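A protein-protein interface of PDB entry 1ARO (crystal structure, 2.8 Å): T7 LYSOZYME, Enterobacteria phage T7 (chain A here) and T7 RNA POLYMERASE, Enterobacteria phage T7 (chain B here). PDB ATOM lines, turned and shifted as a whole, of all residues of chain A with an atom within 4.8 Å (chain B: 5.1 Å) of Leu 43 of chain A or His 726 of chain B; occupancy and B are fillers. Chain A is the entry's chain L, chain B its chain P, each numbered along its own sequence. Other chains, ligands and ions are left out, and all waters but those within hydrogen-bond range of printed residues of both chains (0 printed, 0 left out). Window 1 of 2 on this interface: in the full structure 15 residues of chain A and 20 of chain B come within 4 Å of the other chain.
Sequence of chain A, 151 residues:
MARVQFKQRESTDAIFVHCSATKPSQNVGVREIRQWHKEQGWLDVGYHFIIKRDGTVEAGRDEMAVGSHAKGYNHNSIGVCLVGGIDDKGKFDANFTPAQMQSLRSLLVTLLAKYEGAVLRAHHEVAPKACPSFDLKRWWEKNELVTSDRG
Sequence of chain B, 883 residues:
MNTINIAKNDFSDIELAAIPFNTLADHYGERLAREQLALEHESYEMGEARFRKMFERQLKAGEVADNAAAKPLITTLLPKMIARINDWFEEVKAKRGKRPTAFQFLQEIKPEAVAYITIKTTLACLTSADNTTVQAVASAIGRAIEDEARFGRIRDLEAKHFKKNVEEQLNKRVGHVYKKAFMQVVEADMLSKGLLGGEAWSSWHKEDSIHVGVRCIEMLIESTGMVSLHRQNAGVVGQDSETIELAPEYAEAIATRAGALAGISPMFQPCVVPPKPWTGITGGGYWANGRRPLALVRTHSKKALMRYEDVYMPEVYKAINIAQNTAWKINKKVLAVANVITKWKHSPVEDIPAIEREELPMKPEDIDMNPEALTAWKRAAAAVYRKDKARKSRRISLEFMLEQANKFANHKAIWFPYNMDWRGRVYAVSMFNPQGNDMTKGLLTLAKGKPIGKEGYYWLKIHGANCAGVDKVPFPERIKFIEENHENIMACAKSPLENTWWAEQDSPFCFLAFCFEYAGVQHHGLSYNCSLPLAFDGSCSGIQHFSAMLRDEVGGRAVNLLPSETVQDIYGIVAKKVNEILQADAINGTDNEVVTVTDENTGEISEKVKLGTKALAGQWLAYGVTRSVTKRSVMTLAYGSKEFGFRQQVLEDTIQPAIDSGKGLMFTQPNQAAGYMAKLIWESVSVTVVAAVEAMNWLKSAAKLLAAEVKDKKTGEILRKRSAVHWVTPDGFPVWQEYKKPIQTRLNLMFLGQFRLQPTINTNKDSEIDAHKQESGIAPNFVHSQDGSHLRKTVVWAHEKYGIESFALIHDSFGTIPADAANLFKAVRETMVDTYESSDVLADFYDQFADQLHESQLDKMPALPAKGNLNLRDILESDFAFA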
ATOM      1  N   VAL A   4      -3.297  20.504  -6.618  1.00  0.00           N
ATOM      2  CA  VAL A   4      -4.623  21.096  -6.658  1.00  0.00           C
ATOM      3  C   VAL A   4      -5.483  20.097  -7.420  1.00  0.00           C
ATOM      4  O   VAL A   4      -5.053  19.548  -8.428  1.00  0.00           O
ATOM      5  CB  VAL A   4      -4.587  22.413  -7.410  1.00  0.00           C
ATOM      6  CG1 VAL A   4      -3.730  22.260  -8.640  1.00  0.00           C
ATOM      7  CG2 VAL A   4      -5.972  22.823  -7.821  1.00  0.00           C
ATOM      8  N   PHE A   6      -9.238  19.120  -9.359  1.00  0.00           N
ATOM      9  CA  PHE A   6     -10.419  19.715 -10.015  1.00  0.00           C
ATOM     10  C   PHE A   6     -11.607  18.722  -9.999  1.00  0.00           C
ATOM     11  O   PHE A   6     -11.400  17.504  -9.914  1.00  0.00           O
ATOM     12  CB  PHE A   6     -10.143  20.074 -11.481  1.00  0.00           C
ATOM     13  CG  PHE A   6      -9.001  21.020 -11.686  1.00  0.00           C
ATOM     14  CD1 PHE A   6      -9.207  22.394 -11.674  1.00  0.00           C
ATOM     15  CD2 PHE A   6      -7.714  20.542 -11.874  1.00  0.00           C
ATOM     16  CE1 PHE A   6      -8.142  23.278 -11.845  1.00  0.00           C
ATOM     17  CE2 PHE A   6      -6.637  21.420 -12.047  1.00  0.00           C
ATOM     18  CZ  PHE A   6      -6.856  22.791 -12.031  1.00  0.00           C
ATOM     19  N   LYS A  38      -0.052  29.179 -16.780  1.00  0.00           N
ATOM     20  CA  LYS A  38      -0.021  29.933 -15.541  1.00  0.00           C
ATOM     21  C   LYS A  38      -0.153  31.403 -15.970  1.00  0.00           C
ATOM     22  O   LYS A  38      -0.933  32.170 -15.409  1.00  0.00           O
ATOM     23  CB  LYS A  38       1.291  29.689 -14.811  1.00  0.00           C
ATOM     24  CG  LYS A  38       1.393  30.370 -13.462  1.00  0.00           C
ATOM     25  CD  LYS A  38       2.692  29.983 -12.766  1.00  0.00           C
ATOM     26  CE  LYS A  38       3.882  30.228 -13.671  1.00  0.00           C
ATOM     27  NZ  LYS A  38       5.150  29.626 -13.206  1.00  0.00           N
ATOM     28  N   GLY A  41      -3.234  32.563 -16.834  1.00  0.00           N
ATOM     29  CA  GLY A  41      -3.968  32.658 -15.561  1.00  0.00           C
ATOM     30  C   GLY A  41      -4.598  31.404 -14.921  1.00  0.00           C
ATOM     31  O   GLY A  41      -5.625  31.502 -14.257  1.00  0.00           O
ATOM     32  N   TRP A  42      -3.989  30.232 -15.070  1.00  0.00           N
ATOM     33  CA  TRP A  42      -4.602  29.010 -14.564  1.00  0.00           C
ATOM     34  C   TRP A  42      -3.816  28.177 -13.538  1.00  0.00           C
ATOM     35  O   TRP A  42      -2.606  27.990 -13.675  1.00  0.00           O
ATOM     36  CB  TRP A  42      -4.967  28.116 -15.757  1.00  0.00           C
ATOM     37  CG  TRP A  42      -5.766  28.809 -16.827  1.00  0.00           C
ATOM     38  CD1 TRP A  42      -6.541  29.932 -16.679  1.00  0.00           C
ATOM     39  CD2 TRP A  42      -5.944  28.381 -18.186  1.00  0.00           C
ATOM     40  NE1 TRP A  42      -7.189  30.227 -17.860  1.00  0.00           N
ATOM     41  CE2 TRP A  42      -6.844  29.291 -18.802  1.00  0.00           C
ATOM     42  CE3 TRP A  42      -5.436  27.317 -18.947  1.00  0.00           C
ATOM     43  CZ2 TRP A  42      -7.245  29.166 -20.144  1.00  0.00           C
ATOM     44  CZ3 TRP A  42      -5.840  27.193 -20.295  1.00  0.00           C
ATOM     45  CH2 TRP A  42      -6.735  28.117 -20.870  1.00  0.00           C
ATOM     46  N   LEU A  43      -4.531  27.657 -12.535  1.00  0.00           N
ATOM     47  CA  LEU A  43      -3.965  26.833 -11.466  1.00  0.00           C
ATOM     48  C   LEU A  43      -3.219  25.593 -11.958  1.00  0.00           C
ATOM     49  O   LEU A  43      -2.444  25.003 -11.208  1.00  0.00           O
ATOM     50  CB  LEU A  43      -5.076  26.410 -10.494  1.00  0.00           C
ATOM     51  CG  LEU A  43      -5.747  27.518  -9.656  1.00  0.00           C
ATOM     52  CD1 LEU A  43      -6.999  27.011  -8.904  1.00  0.00           C
ATOM     53  CD2 LEU A  43      -4.705  28.056  -8.679  1.00  0.00           C
ATOM     54  N   ASP A  44      -3.461  25.197 -13.213  1.00  0.00           N
ATOM     55  CA  ASP A  44      -2.786  24.031 -13.808  1.00  0.00           C
ATOM     56  C   ASP A  44      -2.972  23.879 -15.330  1.00  0.00           C
ATOM     57  O   ASP A  44      -3.894  24.427 -15.916  1.00  0.00           O
ATOM     58  CB  ASP A  44      -3.280  22.753 -13.152  1.00  0.00           C
ATOM     59  CG  ASP A  44      -2.276  21.636 -13.248  1.00  0.00           C
ATOM     60  OD1 ASP A  44      -1.374  21.705 -14.117  1.00  0.00           O
ATOM     61  OD2 ASP A  44      -2.402  20.679 -12.452  1.00  0.00           O
ATOM     62  N   ARG B 307     -11.118  31.730 -10.590  1.00  0.00           N
ATOM     63  CA  ARG B 307     -10.275  30.551 -10.734  1.00  0.00           C
ATOM     64  C   ARG B 307     -10.518  29.475  -9.664  1.00  0.00           C
ATOM     65  O   ARG B 307      -9.818  28.466  -9.643  1.00  0.00           O
ATOM     66  CB  ARG B 307      -8.791  30.945 -10.736  1.00  0.00           C
ATOM     67  CG  ARG B 307      -8.273  31.276  -9.372  1.00  0.00           C
ATOM     68  CD  ARG B 307      -6.822  31.698  -9.354  1.00  0.00           C
ATOM     69  NE  ARG B 307      -6.596  33.056  -9.829  1.00  0.00           N
ATOM     70  CZ  ARG B 307      -6.180  33.353 -11.049  1.00  0.00           C
ATOM     71  NH1 ARG B 307      -5.947  32.375 -11.912  1.00  0.00           N
ATOM     72  NH2 ARG B 307      -5.974  34.623 -11.390  1.00  0.00           N
ATOM     73  N   VAL B 311     -12.340  24.162  -8.986  1.00  0.00           N
ATOM     74  CA  VAL B 311     -11.618  23.510  -7.868  1.00  0.00           C
ATOM     75  C   VAL B 311     -12.425  22.647  -6.912  1.00  0.00           C
ATOM     76  O   VAL B 311     -13.410  23.085  -6.365  1.00  0.00           O
ATOM     77  CB  VAL B 311     -10.891  24.554  -7.014  1.00  0.00           C
ATOM     78  CG1 VAL B 311     -10.279  23.902  -5.819  1.00  0.00           C
ATOM     79  CG2 VAL B 311      -9.829  25.226  -7.836  1.00  0.00           C
ATOM     80  N   ALA B 724       3.052  34.969 -11.839  1.00  0.00           N
ATOM     81  CA  ALA B 724       2.425  34.608 -10.581  1.00  0.00           C
ATOM     82  C   ALA B 724       3.124  33.435  -9.888  1.00  0.00           C
ATOM     83  O   ALA B 724       3.902  32.692 -10.491  1.00  0.00           O
ATOM     84  CB  ALA B 724       0.981  34.258 -10.831  1.00  0.00           C
ATOM     85  N   VAL B 725       2.839  33.272  -8.606  1.00  0.00           N
ATOM     86  CA  VAL B 725       3.391  32.174  -7.830  1.00  0.00           C
ATOM     87  C   VAL B 725       2.211  31.617  -7.069  1.00  0.00           C
ATOM     88  O   VAL B 725       1.470  32.387  -6.469  1.00  0.00           O
ATOM     89  CB  VAL B 725       4.430  32.672  -6.831  1.00  0.00           C
ATOM     90  CG1 VAL B 725       4.866  31.531  -5.931  1.00  0.00           C
ATOM     91  CG2 VAL B 725       5.606  33.259  -7.572  1.00  0.00           C
ATOM     92  N   HIS B 726       2.009  30.303  -7.092  1.00  0.00           N
ATOM     93  CA  HIS B 726       0.868  29.729  -6.362  1.00  0.00           C
ATOM     94  C   HIS B 726       1.211  28.489  -5.519  1.00  0.00           C
ATOM     95  O   HIS B 726       2.270  27.893  -5.705  1.00  0.00           O
ATOM     96  CB  HIS B 726      -0.257  29.374  -7.341  1.00  0.00           C
ATOM     97  CG  HIS B 726       0.106  28.287  -8.293  1.00  0.00           C
ATOM     98  ND1 HIS B 726       0.600  27.076  -7.872  1.00  0.00           N
ATOM     99  CD2 HIS B 726       0.102  28.241  -9.644  1.00  0.00           C
ATOM    100  CE1 HIS B 726       0.889  26.327  -8.919  1.00  0.00           C
ATOM    101  NE2 HIS B 726       0.597  27.012 -10.009  1.00  0.00           N
ATOM    102  N   TRP B 727       0.325  28.110  -4.593  1.00  0.00           N
ATOM    103  CA  TRP B 727       0.536  26.902  -3.772  1.00  0.00           C
ATOM    104  C   TRP B 727      -0.723  26.397  -3.061  1.00  0.00           C
ATOM    105  O   TRP B 727      -1.623  27.183  -2.790  1.00  0.00           O
ATOM    106  CB  TRP B 727       1.647  27.149  -2.757  1.00  0.00           C
ATOM    107  CG  TRP B 727       1.327  28.133  -1.736  1.00  0.00           C
ATOM    108  CD1 TRP B 727       0.671  27.907  -0.587  1.00  0.00           C
ATOM    109  CD2 TRP B 727       1.634  29.529  -1.762  1.00  0.00           C
ATOM    110  NE1 TRP B 727       0.545  29.064   0.129  1.00  0.00           N
ATOM    111  CE2 TRP B 727       1.126  30.085  -0.571  1.00  0.00           C
ATOM    112  CE3 TRP B 727       2.288  30.366  -2.677  1.00  0.00           C
ATOM    113  CZ2 TRP B 727       1.248  31.449  -0.254  1.00  0.00           C
ATOM    114  CZ3 TRP B 727       2.412  31.727  -2.366  1.00  0.00           C
ATOM    115  CH2 TRP B 727       1.893  32.253  -1.163  1.00  0.00           C
ATOM    116  N   VAL B 728      -0.796  25.087  -2.784  1.00  0.00           N
ATOM    117  CA  VAL B 728      -1.983  24.524  -2.103  1.00  0.00           C
ATOM    118  C   VAL B 728      -1.841  23.943  -0.698  1.00  0.00           C
ATOM    119  O   VAL B 728      -1.036  23.044  -0.457  1.00  0.00           O
ATOM    120  CB  VAL B 728      -2.666  23.396  -2.900  1.00  0.00           C
ATOM    121  CG1 VAL B 728      -4.182  23.424  -2.605  1.00  0.00           C
ATOM    122  CG2 VAL B 728      -2.396  23.538  -4.377  1.00  0.00           C
ATOM    123  N   PRO B 734      -6.384  26.411  -2.756  1.00  0.00           N
ATOM    124  CA  PRO B 734      -5.368  26.981  -3.656  1.00  0.00           C
ATOM    125  C   PRO B 734      -5.088  28.446  -3.381  1.00  0.00           C
ATOM    126  O   PRO B 734      -6.011  29.243  -3.320  1.00  0.00           O
ATOM    127  CB  PRO B 734      -6.005  26.823  -5.022  1.00  0.00           C
ATOM    128  CG  PRO B 734      -7.256  25.919  -4.752  1.00  0.00           C
ATOM    129  CD  PRO B 734      -7.679  26.414  -3.442  1.00  0.00           C
ATOM    130  N   VAL B 735      -3.828  28.821  -3.239  1.00  0.00           N
ATOM    131  CA  VAL B 735      -3.501  30.222  -2.987  1.00  0.00           C
ATOM    132  C   VAL B 735      -2.737  30.803  -4.169  1.00  0.00           C
ATOM    133  O   VAL B 735      -1.682  30.287  -4.534  1.00  0.00           O
ATOM    134  CB  VAL B 735      -2.615  30.387  -1.721  1.00  0.00           C
ATOM    135  CG1 VAL B 735      -2.409  31.891  -1.405  1.00  0.00           C
ATOM    136  CG2 VAL B 735      -3.229  29.626  -0.553  1.00  0.00           C
ATOM    137  N   TRP B 736      -3.260  31.884  -4.748  1.00  0.00           N
ATOM    138  CA  TRP B 736      -2.641  32.557  -5.905  1.00  0.00           C
ATOM    139  C   TRP B 736      -2.096  33.975  -5.575  1.00  0.00           C
ATOM    140  O   TRP B 736      -2.864  34.921  -5.381  1.00  0.00           O
ATOM    141  CB  TRP B 736      -3.677  32.623  -7.032  1.00  0.00           C
ATOM    142  CG  TRP B 736      -3.219  33.244  -8.309  1.00  0.00           C
ATOM    143  CD1 TRP B 736      -3.064  34.578  -8.578  1.00  0.00           C
ATOM    144  CD2 TRP B 736      -2.870  32.547  -9.511  1.00  0.00           C
ATOM    145  NE1 TRP B 736      -2.644  34.748  -9.883  1.00  0.00           N
ATOM    146  CE2 TRP B 736      -2.520  33.517 -10.475  1.00  0.00           C
ATOM    147  CE3 TRP B 736      -2.821  31.198  -9.865  1.00  0.00           C
ATOM    148  CZ2 TRP B 736      -2.128  33.175 -11.768  1.00  0.00           C
ATOM    149  CZ3 TRP B 736      -2.436  30.861 -11.149  1.00  0.00           C
ATOM    150  CH2 TRP B 736      -2.093  31.846 -12.090  1.00  0.00           C
ATOM    151  N   GLN B 737      -0.773  34.123  -5.508  1.00  0.00           N
ATOM    152  CA  GLN B 737      -0.183  35.432  -5.202  1.00  0.00           C
ATOM    153  C   GLN B 737       0.379  36.112  -6.447  1.00  0.00           C
ATOM    154  O   GLN B 737       1.270  35.586  -7.109  1.00  0.00           O
ATOM    155  CB  GLN B 737       0.929  35.302  -4.182  1.00  0.00           C
ATOM    156  CG  GLN B 737       1.433  36.640  -3.799  1.00  0.00           C
ATOM    157  CD  GLN B 737       2.625  36.556  -2.924  1.00  0.00           C
ATOM    158  OE1 GLN B 737       3.610  35.914  -3.276  1.00  0.00           O
ATOM    159  NE2 GLN B 737       2.559  37.209  -1.771  1.00  0.00           N
ATOM    160  N   PHE B 849       6.683  23.619  -5.696  1.00  0.00           N
ATOM    161  CA  PHE B 849       7.367  24.798  -6.187  1.00  0.00           C
ATOM    162  C   PHE B 849       8.218  24.412  -7.386  1.00  0.00           C
ATOM    163  O   PHE B 849       8.144  25.048  -8.444  1.00  0.00           O
ATOM    164  CB  PHE B 849       8.213  25.395  -5.054  1.00  0.00           C
ATOM    165  CG  PHE B 849       7.393  26.059  -3.952  1.00  0.00           C
ATOM    166  CD1 PHE B 849       6.156  26.652  -4.233  1.00  0.00           C
ATOM    167  CD2 PHE B 849       7.907  26.170  -2.656  1.00  0.00           C
ATOM    168  CE1 PHE B 849       5.459  27.346  -3.247  1.00  0.00           C
ATOM    169  CE2 PHE B 849       7.209  26.864  -1.669  1.00  0.00           C
ATOM    170  CZ  PHE B 849       5.986  27.454  -1.965  1.00  0.00           C
ATOM    171  N   GLN B 852       7.029  24.677 -10.839  1.00  0.00           N
ATOM    172  CA  GLN B 852       6.767  25.961 -11.458  1.00  0.00           C
ATOM    173  C   GLN B 852       8.026  26.654 -11.952  1.00  0.00           C
ATOM    174  O   GLN B 852       8.017  27.871 -12.145  1.00  0.00           O
ATOM    175  CB  GLN B 852       6.072  26.870 -10.442  1.00  0.00           C
ATOM    176  CG  GLN B 852       4.908  26.246  -9.719  1.00  0.00           C
ATOM    177  CD  GLN B 852       4.276  27.208  -8.754  1.00  0.00           C
ATOM    178  OE1 GLN B 852       3.875  28.292  -9.135  1.00  0.00           O
ATOM    179  NE2 GLN B 852       4.185  26.820  -7.499  1.00  0.00           N
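The guanidinium group (NH1) of Arg 307 of chain B lies within hydrogen-bond range of the backbone carbonyl oxygen (O) of Gly 41 of chain A, at 2.5 Å.
The backbone carbonyl oxygen (O) of His 726 of chain B is in hydrogen-bond range of the side-chain amide nitrogen (NE2) of Gln 852 of chain B (2.8 Å).
N of Val 4 of chain A touches CG2 of Val 728 of chain B, at 3.9 Å.
Ala 724 of chain B touches Lys 38 of chain A (O to CD, 3.7 Å).
O of Lys 38 of chain A touches CH2 of Trp 736 of chain B, at 3.5 Å.
Gln 852 of chain B touches Lys 38 of chain A.
Gly 41 of chain A touches Trp 736 of chain B.
Trp 736 of chain B touches Trp 42 of chain A.
CD1 of Leu 43 of chain A touches O of Arg 307 of chain B, at 3.3 Å.
CD1 of Leu 43 of chain A touches CG2 of Val 311 of chain B, at 3.5 Å.
His 726 of chain B touches Leu 43 of chain A.
Leu 43 of chain A touches Trp 736 of chain B.
Of the printed residues of chain B, Lys 38 of chain A touches Ala 724 (3.7 Å), Trp 736 (3.5 Å) and Gln 852 (3.5 Å).
Of the printed residues of chain B, Gly 41 of chain A touches Arg 307 and Trp 736.
Printed residues of chain B within 4 Å of Leu 43 of chain A: Arg 307 (3.3 Å), Val 311 (3.5 Å), His 726 (3.8 Å) and Trp 736 (3.9 Å).
His 726 of chain B touches one residue of chain A.
The nearest printed residue of chain B that does not touch Leu 43 of chain A is Pro 734 of chain B (4.01 Å).
The nearest printed residue of chain B that does not touch Lys 38 of chain A is His 726 of chain B (4.4 Å).
Of the 7 printed residues of chain A, 5 touch a printed residue of chain B.
Of the 13 printed residues of chain B, 7 touch a printed residue of chain A.
Hydrophobic or aromatic side chains of chain B within 4 Å of the printed part of chain A: Val 311, His 726, Val 728 and Trp 736.
Among the printed residues, 11 pairs touch across the chains.
Among the printed residues, no Asp or Glu carboxylate lies within 4 Å of a Lys or Arg side-chain nitrogen of the other chain.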
